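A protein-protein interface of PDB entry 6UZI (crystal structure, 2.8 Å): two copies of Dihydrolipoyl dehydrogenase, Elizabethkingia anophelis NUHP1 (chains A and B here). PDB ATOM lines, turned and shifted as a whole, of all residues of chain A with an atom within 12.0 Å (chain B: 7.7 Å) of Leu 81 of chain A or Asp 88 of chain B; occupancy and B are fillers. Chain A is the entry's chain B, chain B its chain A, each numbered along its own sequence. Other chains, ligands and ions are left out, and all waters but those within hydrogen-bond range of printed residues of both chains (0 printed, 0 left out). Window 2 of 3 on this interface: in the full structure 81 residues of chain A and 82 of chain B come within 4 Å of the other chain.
Ile 82 of chain B touches its own counterpart, Ile 82 of chain A. Ile 82 of chain A touches Pro 85 of chain B, and with the chains exchanged Pro 85 of chain A touches Ile 82 of chain B. Asp 83 of chain B touches its own counterpart, Asp 83 of chain A. Of the 15 pairs that touch across the chains among the printed residues, 4 have their exchanged pair printed and touching as well.
Of the printed residues of chain B, Ala 76 of chain A touches Gln 91 (3.3 Å). Glu 84 of chain A touches none of the printed residues of chain B. Printed residues of chain B within 4 Å of Pro 85 of chain A: Ile 82. Pro 85 of chain B touches just these residues of chain A: Leu 81 (3.6 Å) and Ile 82 (3.7 Å). Val 87 of chain B touches just one residue of chain A: Gly 79. Asp 88 of chain B touches just these residues of chain A: Gly 79 and Leu 81. Ile 89 of chain B touches none of the printed residues of chain A. Of chain A, only Ala 76, Thr 77 and Gly 79 come within 4 Å of Gln 91 of chain B. Met 92 of chain B touches just one residue of chain A: His 78 (3.0 Å). Val 181 of chain B touches none of the printed residues of chain A. The nearest residue of chain B that does not touch Leu 81 of chain A is Val 87 of chain B (4.3 Å). The nearest residue of chain A that does not touch Asp 88 of chain B is Ile 80 of chain A (4.8 Å). The nearest printed residue of chain B that does not touch Gly 79 of chain A is Lys 86 of chain B (4.04 Å).
The backbone NH of Ala 90 of chain B lies close to the side-chain carboxylate of Asp 88 of chain B. The backbone NH of Ile 80 of chain A sits at hydrogen-bond distance from the backbone carbonyl oxygen of Phe 75 of chain A.
Among the printed residues, merely in contact across the chains: His 78 of chain A with Met 92 of chain B (3.0 Å), Ala 76 of chain A with Gln 91 of chain B (3.3 Å), Ile 80 of chain A with Phe 68 of chain B (3.4 Å), Leu 81 of chain A with Pro 85 of chain B (3.6 Å), Gly 79 of chain A with Gln 91 of chain B (3.6 Å), Ile 80 of chain A with Lys 86 of chain B (3.6 Å), Ile 82 of chain A with Pro 85 of chain B (3.7 Å), Pro 85 of chain A with Ile 82 of chain B (3.7 Å), Gly 79 of chain A with Val 87 of chain B (3.8 Å), Leu 81 of chain A with Asp 88 of chain B (3.8 Å) and Ile 82 of chain A with Ile 82 of chain B (3.98 Å).
The backbone carbonyl oxygen of Lys 86 of chain B is in hydrogen-bond range of the backbone NH of Leu 81 of chain A (2.7 Å). N of Asp 88 of chain B sits at hydrogen-bond distance from O of Gly 79 of chain A (2.8 Å). O of Thr 77 of chain A lies within hydrogen-bond range of NE2 of Gln 91 of chain B. OD1 of Asp 83 of chain A sits close to OD1 of Asp 83 of chain B (2.9 Å).
Of the 17 printed residues of chain A, 9 touch a printed residue of chain B. Printed residues of chain B that touch a printed residue of chain A: Phe 68, Ile 82, Asp 83, Pro 85, Lys 86, Val 87, Asp 88, Gln 91 and Met 92. Among the printed residues, 15 pairs touch across the chains.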
ATOM      1  N   ASN A  70       7.312  26.236 -20.368  1.00  0.00           N
ATOM      2  CA  ASN A  70       7.457  26.388 -21.816  1.00  0.00           C
ATOM      3  C   ASN A  70       7.628  25.041 -22.500  1.00  0.00           C
ATOM      4  O   ASN A  70       6.943  24.740 -23.483  1.00  0.00           O
ATOM      5  CB  ASN A  70       8.649  27.287 -22.149  1.00  0.00           C
ATOM      6  CG  ASN A  70       8.411  28.725 -21.785  1.00  0.00           C
ATOM      7  OD1 ASN A  70       7.334  29.261 -22.026  1.00  0.00           O
ATOM      8  ND2 ASN A  70       9.415  29.363 -21.198  1.00  0.00           N
ATOM      9  N   ALA A  71       8.538  24.216 -21.986  1.00  0.00           N
ATOM     10  CA  ALA A  71       8.776  22.914 -22.592  1.00  0.00           C
ATOM     11  C   ALA A  71       7.503  22.087 -22.646  1.00  0.00           C
ATOM     12  O   ALA A  71       7.311  21.304 -23.583  1.00  0.00           O
ATOM     13  CB  ALA A  71       9.869  22.174 -21.822  1.00  0.00           C
ATOM     14  N   LYS A  72       6.625  22.241 -21.654  1.00  0.00           N
ATOM     15  CA  LYS A  72       5.427  21.414 -21.589  1.00  0.00           C
ATOM     16  C   LYS A  72       4.290  21.939 -22.460  1.00  0.00           C
ATOM     17  O   LYS A  72       3.504  21.136 -22.973  1.00  0.00           O
ATOM     18  CB  LYS A  72       4.965  21.297 -20.136  1.00  0.00           C
ATOM     19  CG  LYS A  72       3.915  20.236 -19.891  1.00  0.00           C
ATOM     20  CD  LYS A  72       3.593  20.129 -18.413  1.00  0.00           C
ATOM     21  CE  LYS A  72       2.390  19.224 -18.163  1.00  0.00           C
ATOM     22  NZ  LYS A  72       2.078  19.109 -16.705  1.00  0.00           N
ATOM     23  N   HIS A  73       4.193  23.260 -22.665  1.00  0.00           N
ATOM     24  CA  HIS A  73       3.009  23.847 -23.287  1.00  0.00           C
ATOM     25  C   HIS A  73       3.260  24.714 -24.514  1.00  0.00           C
ATOM     26  O   HIS A  73       2.314  24.937 -25.278  1.00  0.00           O
ATOM     27  CB  HIS A  73       2.226  24.689 -22.267  1.00  0.00           C
ATOM     28  CG  HIS A  73       1.566  23.877 -21.199  1.00  0.00           C
ATOM     29  ND1 HIS A  73       1.394  24.338 -19.912  1.00  0.00           N
ATOM     30  CD2 HIS A  73       1.047  22.626 -21.225  1.00  0.00           C
ATOM     31  CE1 HIS A  73       0.793  23.407 -19.191  1.00  0.00           C
ATOM     32  NE2 HIS A  73       0.572  22.358 -19.965  1.00  0.00           N
ATOM     33  N   THR A  74       4.479  25.219 -24.730  1.00  0.00           N
ATOM     34  CA  THR A  74       4.715  26.143 -25.832  1.00  0.00           C
ATOM     35  C   THR A  74       5.794  25.698 -26.811  1.00  0.00           C
ATOM     36  O   THR A  74       5.836  26.225 -27.931  1.00  0.00           O
ATOM     37  CB  THR A  74       5.083  27.541 -25.298  1.00  0.00           C
ATOM     38  OG1 THR A  74       6.320  27.480 -24.581  1.00  0.00           O
ATOM     39  CG2 THR A  74       4.001  28.065 -24.373  1.00  0.00           C
ATOM     40  N   PHE A  75       6.629  24.718 -26.451  1.00  0.00           N
ATOM     41  CA  PHE A  75       7.742  24.337 -27.315  1.00  0.00           C
ATOM     42  C   PHE A  75       7.254  23.818 -28.660  1.00  0.00           C
ATOM     43  O   PHE A  75       7.833  24.139 -29.702  1.00  0.00           O
ATOM     44  CB  PHE A  75       8.600  23.275 -26.628  1.00  0.00           C
ATOM     45  CG  PHE A  75       9.734  23.830 -25.831  1.00  0.00           C
ATOM     46  CD1 PHE A  75      10.778  23.009 -25.428  1.00  0.00           C
ATOM     47  CD2 PHE A  75       9.754  25.163 -25.464  1.00  0.00           C
ATOM     48  CE1 PHE A  75      11.830  23.515 -24.678  1.00  0.00           C
ATOM     49  CE2 PHE A  75      10.807  25.677 -24.723  1.00  0.00           C
ATOM     50  CZ  PHE A  75      11.844  24.852 -24.327  1.00  0.00           C
ATOM     51  N   ALA A  76       6.170  23.038 -28.659  1.00  0.00           N
ATOM     52  CA  ALA A  76       5.649  22.495 -29.909  1.00  0.00           C
ATOM     53  C   ALA A  76       5.232  23.605 -30.865  1.00  0.00           C
ATOM     54  O   ALA A  76       5.542  23.552 -32.063  1.00  0.00           O
ATOM     55  CB  ALA A  76       4.475  21.565 -29.619  1.00  0.00           C
ATOM     56  N   THR A  77       4.527  24.620 -30.356  1.00  0.00           N
ATOM     57  CA  THR A  77       4.191  25.776 -31.180  1.00  0.00           C
ATOM     58  C   THR A  77       5.450  26.506 -31.619  1.00  0.00           C
ATOM     59  O   THR A  77       5.534  27.008 -32.750  1.00  0.00           O
ATOM     60  CB  THR A  77       3.257  26.715 -30.418  1.00  0.00           C
ATOM     61  OG1 THR A  77       2.088  25.995 -30.012  1.00  0.00           O
ATOM     62  CG2 THR A  77       2.855  27.890 -31.281  1.00  0.00           C
ATOM     63  N   HIS A  78       6.449  26.560 -30.743  1.00  0.00           N
ATOM     64  CA  HIS A  78       7.706  27.202 -31.080  1.00  0.00           C
ATOM     65  C   HIS A  78       8.519  26.427 -32.107  1.00  0.00           C
ATOM     66  O   HIS A  78       9.516  26.963 -32.595  1.00  0.00           O
ATOM     67  CB  HIS A  78       8.554  27.377 -29.823  1.00  0.00           C
ATOM     68  CG  HIS A  78       8.304  28.659 -29.100  1.00  0.00           C
ATOM     69  ND1 HIS A  78       8.426  29.889 -29.708  1.00  0.00           N
ATOM     70  CD2 HIS A  78       7.963  28.904 -27.812  1.00  0.00           C
ATOM     71  CE1 HIS A  78       8.156  30.837 -28.828  1.00  0.00           C
ATOM     72  NE2 HIS A  78       7.878  30.267 -27.669  1.00  0.00           N
ATOM     73  N   GLY A  79       8.123  25.205 -32.457  1.00  0.00           N
ATOM     74  CA  GLY A  79       8.922  24.435 -33.388  1.00  0.00           C
ATOM     75  C   GLY A  79      10.075  23.690 -32.758  1.00  0.00           C
ATOM     76  O   GLY A  79      11.048  23.381 -33.450  1.00  0.00           O
ATOM     77  N   ILE A  80      10.004  23.413 -31.459  1.00  0.00           N
ATOM     78  CA  ILE A  80      11.026  22.675 -30.724  1.00  0.00           C
ATOM     79  C   ILE A  80      10.467  21.297 -30.399  1.00  0.00           C
ATOM     80  O   ILE A  80       9.430  21.182 -29.732  1.00  0.00           O
ATOM     81  CB  ILE A  80      11.447  23.429 -29.453  1.00  0.00           C
ATOM     82  CG1 ILE A  80      12.007  24.801 -29.834  1.00  0.00           C
ATOM     83  CG2 ILE A  80      12.450  22.625 -28.633  1.00  0.00           C
ATOM     84  CD1 ILE A  80      12.224  25.709 -28.663  1.00  0.00           C
ATOM     85  N   LEU A  81      11.148  20.251 -30.871  1.00  0.00           N
ATOM     86  CA  LEU A  81      10.676  18.877 -30.733  1.00  0.00           C
ATOM     87  C   LEU A  81      11.347  18.206 -29.542  1.00  0.00           C
ATOM     88  O   LEU A  81      12.551  17.936 -29.571  1.00  0.00           O
ATOM     89  CB  LEU A  81      10.940  18.090 -32.015  1.00  0.00           C
ATOM     90  CG  LEU A  81      10.328  18.672 -33.290  1.00  0.00           C
ATOM     91  CD1 LEU A  81      10.861  17.968 -34.533  1.00  0.00           C
ATOM     92  CD2 LEU A  81       8.803  18.596 -33.228  1.00  0.00           C
ATOM     93  N   ILE A  82      10.560  17.927 -28.500  1.00  0.00           N
ATOM     94  CA  ILE A  82      11.006  17.157 -27.346  1.00  0.00           C
ATOM     95  C   ILE A  82       9.875  16.232 -26.921  1.00  0.00           C
ATOM     96  O   ILE A  82       8.720  16.395 -27.320  1.00  0.00           O
ATOM     97  CB  ILE A  82      11.428  18.040 -26.146  1.00  0.00           C
ATOM     98  CG1 ILE A  82      10.287  18.967 -25.737  1.00  0.00           C
ATOM     99  CG2 ILE A  82      12.681  18.850 -26.457  1.00  0.00           C
ATOM    100  CD1 ILE A  82      10.416  19.480 -24.334  1.00  0.00           C
ATOM    101  N   ASP A  83      10.216  15.250 -26.097  1.00  0.00           N
ATOM    102  CA  ASP A  83       9.192  14.446 -25.458  1.00  0.00           C
ATOM    103  C   ASP A  83       8.727  15.164 -24.192  1.00  0.00           C
ATOM    104  O   ASP A  83       9.197  16.257 -23.864  1.00  0.00           O
ATOM    105  CB  ASP A  83       9.719  13.042 -25.165  1.00  0.00           C
ATOM    106  CG  ASP A  83      11.078  13.053 -24.482  1.00  0.00           C
ATOM    107  OD1 ASP A  83      11.552  14.149 -24.110  1.00  0.00           O
ATOM    108  OD2 ASP A  83      11.676  11.964 -24.330  1.00  0.00           O
ATOM    109  N   GLU A  84       7.760  14.577 -23.499  1.00  0.00           N
ATOM    110  CA  GLU A  84       7.231  15.171 -22.283  1.00  0.00           C
ATOM    111  C   GLU A  84       8.366  15.455 -21.297  1.00  0.00           C
ATOM    112  O   GLU A  84       9.109  14.529 -20.934  1.00  0.00           O
ATOM    113  CB  GLU A  84       6.193  14.247 -21.647  1.00  0.00           C
ATOM    114  N   PRO A  85       8.563  16.705 -20.885  1.00  0.00           N
ATOM    115  CA  PRO A  85       9.626  17.000 -19.920  1.00  0.00           C
ATOM    116  C   PRO A  85       9.280  16.473 -18.536  1.00  0.00           C
ATOM    117  O   PRO A  85       8.112  16.418 -18.137  1.00  0.00           O
ATOM    118  CB  PRO A  85       9.700  18.532 -19.932  1.00  0.00           C
ATOM    119  CG  PRO A  85       8.336  18.965 -20.341  1.00  0.00           C
ATOM    120  CD  PRO A  85       7.847  17.923 -21.308  1.00  0.00           C
ATOM    121  N   LYS A  86      10.319  16.079 -17.802  1.00  0.00           N
ATOM    122  CA  LYS A  86      10.179  15.555 -16.451  1.00  0.00           C
ATOM    123  C   LYS A  86      10.992  16.413 -15.483  1.00  0.00           C
ATOM    124  O   LYS A  86      12.004  17.012 -15.861  1.00  0.00           O
ATOM    125  CB  LYS A  86      10.621  14.082 -16.386  1.00  0.00           C
ATOM    126  N   PHE B  68      15.143  27.232 -27.676  1.00  0.00           N
ATOM    127  CA  PHE B  68      15.914  26.060 -28.080  1.00  0.00           C
ATOM    128  C   PHE B  68      17.309  26.070 -27.464  1.00  0.00           C
ATOM    129  O   PHE B  68      17.833  25.018 -27.074  1.00  0.00           O
ATOM    130  CB  PHE B  68      15.997  25.995 -29.608  1.00  0.00           C
ATOM    131  CG  PHE B  68      16.746  24.794 -30.127  1.00  0.00           C
ATOM    132  CD1 PHE B  68      16.146  23.546 -30.171  1.00  0.00           C
ATOM    133  CD2 PHE B  68      18.056  24.917 -30.570  1.00  0.00           C
ATOM    134  CE1 PHE B  68      16.840  22.439 -30.645  1.00  0.00           C
ATOM    135  CE2 PHE B  68      18.751  23.815 -31.043  1.00  0.00           C
ATOM    136  CZ  PHE B  68      18.137  22.576 -31.084  1.00  0.00           C
ATOM    137  N   ILE B  82      15.058  16.208 -20.221  1.00  0.00           N
ATOM    138  CA  ILE B  82      14.573  15.999 -21.580  1.00  0.00           C
ATOM    139  C   ILE B  82      15.676  15.316 -22.371  1.00  0.00           C
ATOM    140  O   ILE B  82      16.833  15.265 -21.951  1.00  0.00           O
ATOM    141  CB  ILE B  82      14.166  17.309 -22.297  1.00  0.00           C
ATOM    142  CG1 ILE B  82      15.334  18.301 -22.299  1.00  0.00           C
ATOM    143  CG2 ILE B  82      12.924  17.916 -21.667  1.00  0.00           C
ATOM    144  CD1 ILE B  82      15.228  19.358 -23.361  1.00  0.00           C
ATOM    145  N   ASP B  83      15.301  14.773 -23.523  1.00  0.00           N
ATOM    146  CA  ASP B  83      16.286  14.261 -24.461  1.00  0.00           C
ATOM    147  C   ASP B  83      16.756  15.410 -25.349  1.00  0.00           C
ATOM    148  O   ASP B  83      16.281  16.542 -25.235  1.00  0.00           O
ATOM    149  CB  ASP B  83      15.711  13.097 -25.272  1.00  0.00           C
ATOM    150  CG  ASP B  83      14.347  13.410 -25.867  1.00  0.00           C
ATOM    151  OD1 ASP B  83      13.902  14.574 -25.772  1.00  0.00           O
ATOM    152  OD2 ASP B  83      13.711  12.488 -26.422  1.00  0.00           O
ATOM    153  N   GLU B  84      17.712  15.124 -26.230  1.00  0.00           N
ATOM    154  CA  GLU B  84      18.257  16.135 -27.122  1.00  0.00           C
ATOM    155  C   GLU B  84      17.128  16.802 -27.906  1.00  0.00           C
ATOM    156  O   GLU B  84      16.399  16.112 -28.637  1.00  0.00           O
ATOM    157  CB  GLU B  84      19.271  15.510 -28.076  1.00  0.00           C
ATOM    158  CG  GLU B  84      20.725  15.732 -27.669  1.00  0.00           C
ATOM    159  CD  GLU B  84      21.262  17.079 -28.127  1.00  0.00           C
ATOM    160  OE1 GLU B  84      21.576  17.212 -29.332  1.00  0.00           O
ATOM    161  OE2 GLU B  84      21.361  18.004 -27.288  1.00  0.00           O
ATOM    162  N   PRO B  85      16.940  18.115 -27.770  1.00  0.00           N
ATOM    163  CA  PRO B  85      15.868  18.787 -28.512  1.00  0.00           C
ATOM    164  C   PRO B  85      16.203  18.868 -29.990  1.00  0.00           C
ATOM    165  O   PRO B  85      17.367  18.968 -30.379  1.00  0.00           O
ATOM    166  CB  PRO B  85      15.813  20.180 -27.873  1.00  0.00           C
ATOM    167  CG  PRO B  85      17.189  20.396 -27.349  1.00  0.00           C
ATOM    168  CD  PRO B  85      17.682  19.048 -26.904  1.00  0.00           C
ATOM    169  N   LYS B  86      15.162  18.795 -30.815  1.00  0.00           N
ATOM    170  CA  LYS B  86      15.301  18.839 -32.263  1.00  0.00           C
ATOM    171  C   LYS B  86      14.468  19.987 -32.818  1.00  0.00           C
ATOM    172  O   LYS B  86      13.438  20.358 -32.247  1.00  0.00           O
ATOM    173  CB  LYS B  86      14.884  17.502 -32.909  1.00  0.00           C
ATOM    174  N   VAL B  87      14.923  20.549 -33.937  1.00  0.00           N
ATOM    175  CA  VAL B  87      14.313  21.738 -34.522  1.00  0.00           C
ATOM    176  C   VAL B  87      13.326  21.315 -35.602  1.00  0.00           C
ATOM    177  O   VAL B  87      13.696  20.615 -36.552  1.00  0.00           O
ATOM    178  CB  VAL B  87      15.369  22.687 -35.109  1.00  0.00           C
ATOM    179  CG1 VAL B  87      14.684  23.877 -35.760  1.00  0.00           C
ATOM    180  CG2 VAL B  87      16.362  23.136 -34.047  1.00  0.00           C
ATOM    181  N   ASP B  88      12.075  21.755 -35.467  1.00  0.00           N
ATOM    182  CA  ASP B  88      11.079  21.688 -36.538  1.00  0.00           C
ATOM    183  C   ASP B  88      11.040  23.071 -37.180  1.00  0.00           C
ATOM    184  O   ASP B  88      10.289  23.955 -36.760  1.00  0.00           O
ATOM    185  CB  ASP B  88       9.713  21.262 -36.013  1.00  0.00           C
ATOM    186  CG  ASP B  88       8.714  21.006 -37.131  1.00  0.00           C
ATOM    187  OD1 ASP B  88       9.052  21.262 -38.306  1.00  0.00           O
ATOM    188  OD2 ASP B  88       7.582  20.566 -36.836  1.00  0.00           O
ATOM    189  N   ILE B  89      11.886  23.267 -38.192  1.00  0.00           N
ATOM    190  CA  ILE B  89      12.041  24.598 -38.769  1.00  0.00           C
ATOM    191  C   ILE B  89      10.748  25.051 -39.439  1.00  0.00           C
ATOM    192  O   ILE B  89      10.420  26.243 -39.425  1.00  0.00           O
ATOM    193  CB  ILE B  89      13.238  24.628 -39.741  1.00  0.00           C
ATOM    194  CG1 ILE B  89      13.526  26.057 -40.188  1.00  0.00           C
ATOM    195  CG2 ILE B  89      12.967  23.796 -40.972  1.00  0.00           C
ATOM    196  CD1 ILE B  89      13.833  26.979 -39.036  1.00  0.00           C
ATOM    197  N   ALA B  90       9.979  24.123 -40.016  1.00  0.00           N
ATOM    198  CA  ALA B  90       8.745  24.521 -40.687  1.00  0.00           C
ATOM    199  C   ALA B  90       7.750  25.097 -39.696  1.00  0.00           C
ATOM    200  O   ALA B  90       7.029  26.051 -40.012  1.00  0.00           O
ATOM    201  CB  ALA B  90       8.135  23.340 -41.434  1.00  0.00           C
ATOM    202  N   GLN B  91       7.703  24.540 -38.485  1.00  0.00           N
ATOM    203  CA  GLN B  91       6.805  25.078 -37.471  1.00  0.00           C
ATOM    204  C   GLN B  91       7.307  26.424 -36.957  1.00  0.00           C
ATOM    205  O   GLN B  91       6.507  27.324 -36.680  1.00  0.00           O
ATOM    206  CB  GLN B  91       6.636  24.071 -36.331  1.00  0.00           C
ATOM    207  CG  GLN B  91       5.791  24.563 -35.161  1.00  0.00           C
ATOM    208  CD  GLN B  91       4.397  25.028 -35.571  1.00  0.00           C
ATOM    209  OE1 GLN B  91       3.796  24.509 -36.513  1.00  0.00           O
ATOM    210  NE2 GLN B  91       3.883  26.021 -34.859  1.00  0.00           N
ATOM    211  N   MET B  92       8.626  26.582 -36.821  1.00  0.00           N
ATOM    212  CA  MET B  92       9.171  27.881 -36.435  1.00  0.00           C
ATOM    213  C   MET B  92       8.762  28.954 -37.431  1.00  0.00           C
ATOM    214  O   MET B  92       8.178  29.977 -37.058  1.00  0.00           O
ATOM    215  CB  MET B  92      10.695  27.830 -36.342  1.00  0.00           C
ATOM    216  CG  MET B  92      11.219  27.509 -34.988  1.00  0.00           C
ATOM    217  SD  MET B  92      12.816  28.250 -34.653  1.00  0.00           S
ATOM    218  CE  MET B  92      13.241  27.373 -33.153  1.00  0.00           C
ATOM    219  N   ILE B  93       9.048  28.723 -38.712  1.00  0.00           N
ATOM    220  CA  ILE B  93       8.742  29.724 -39.725  1.00  0.00           C
ATOM    221  C   ILE B  93       7.239  29.946 -39.799  1.00  0.00           C
ATOM    222  O   ILE B  93       6.763  31.089 -39.842  1.00  0.00           O
ATOM    223  CB  ILE B  93       9.318  29.297 -41.091  1.00  0.00           C
ATOM    224  CG1 ILE B  93      10.800  28.924 -40.970  1.00  0.00           C
ATOM    225  CG2 ILE B  93       9.161  30.416 -42.090  1.00  0.00           C
ATOM    226  CD1 ILE B  93      11.706  30.071 -40.596  1.00  0.00           C
ATOM    227  N   SER B  94       6.469  28.858 -39.747  1.00  0.00           N
ATOM    228  CA  SER B  94       5.020  28.979 -39.831  1.00  0.00           C
ATOM    229  C   SER B  94       4.471  29.813 -38.686  1.00  0.00           C
ATOM    230  O   SER B  94       3.632  30.695 -38.908  1.00  0.00           O
ATOM    231  CB  SER B  94       4.373  27.596 -39.843  1.00  0.00           C
ATOM    232  OG  SER B  94       2.962  27.708 -39.801  1.00  0.00           O
ATOM    233  N   VAL B 181      17.857  24.365 -41.275  1.00  0.00           N
ATOM    234  CA  VAL B 181      18.869  25.029 -40.456  1.00  0.00           C
ATOM    235  C   VAL B 181      20.206  24.919 -41.179  1.00  0.00           C
ATOM    236  O   VAL B 181      20.651  23.800 -41.475  1.00  0.00           O
ATOM    237  CB  VAL B 181      18.968  24.414 -39.054  1.00  0.00           C
ATOM    238  CG1 VAL B 181      20.189  24.979 -38.330  1.00  0.00           C
ATOM    239  CG2 VAL B 181      17.687  24.670 -38.264  1.00  0.00           C
ATOM    240  N   LEU B 204      20.300  27.390 -33.309  1.00  0.00           N
ATOM    241  CA  LEU B 204      19.649  26.218 -33.890  1.00  0.00           C
ATOM    242  C   LEU B 204      20.622  25.169 -34.422  1.00  0.00           C
ATOM    243  O   LEU B 204      20.174  24.191 -35.028  1.00  0.00           O
ATOM    244  CB  LEU B 204      18.705  26.640 -35.014  1.00  0.00           C
ATOM    245  CG  LEU B 204      17.526  27.553 -34.681  1.00  0.00           C
ATOM    246  CD1 LEU B 204      16.611  27.662 -35.895  1.00  0.00           C
ATOM    247  CD2 LEU B 204      16.754  27.064 -33.455  1.00  0.00           C
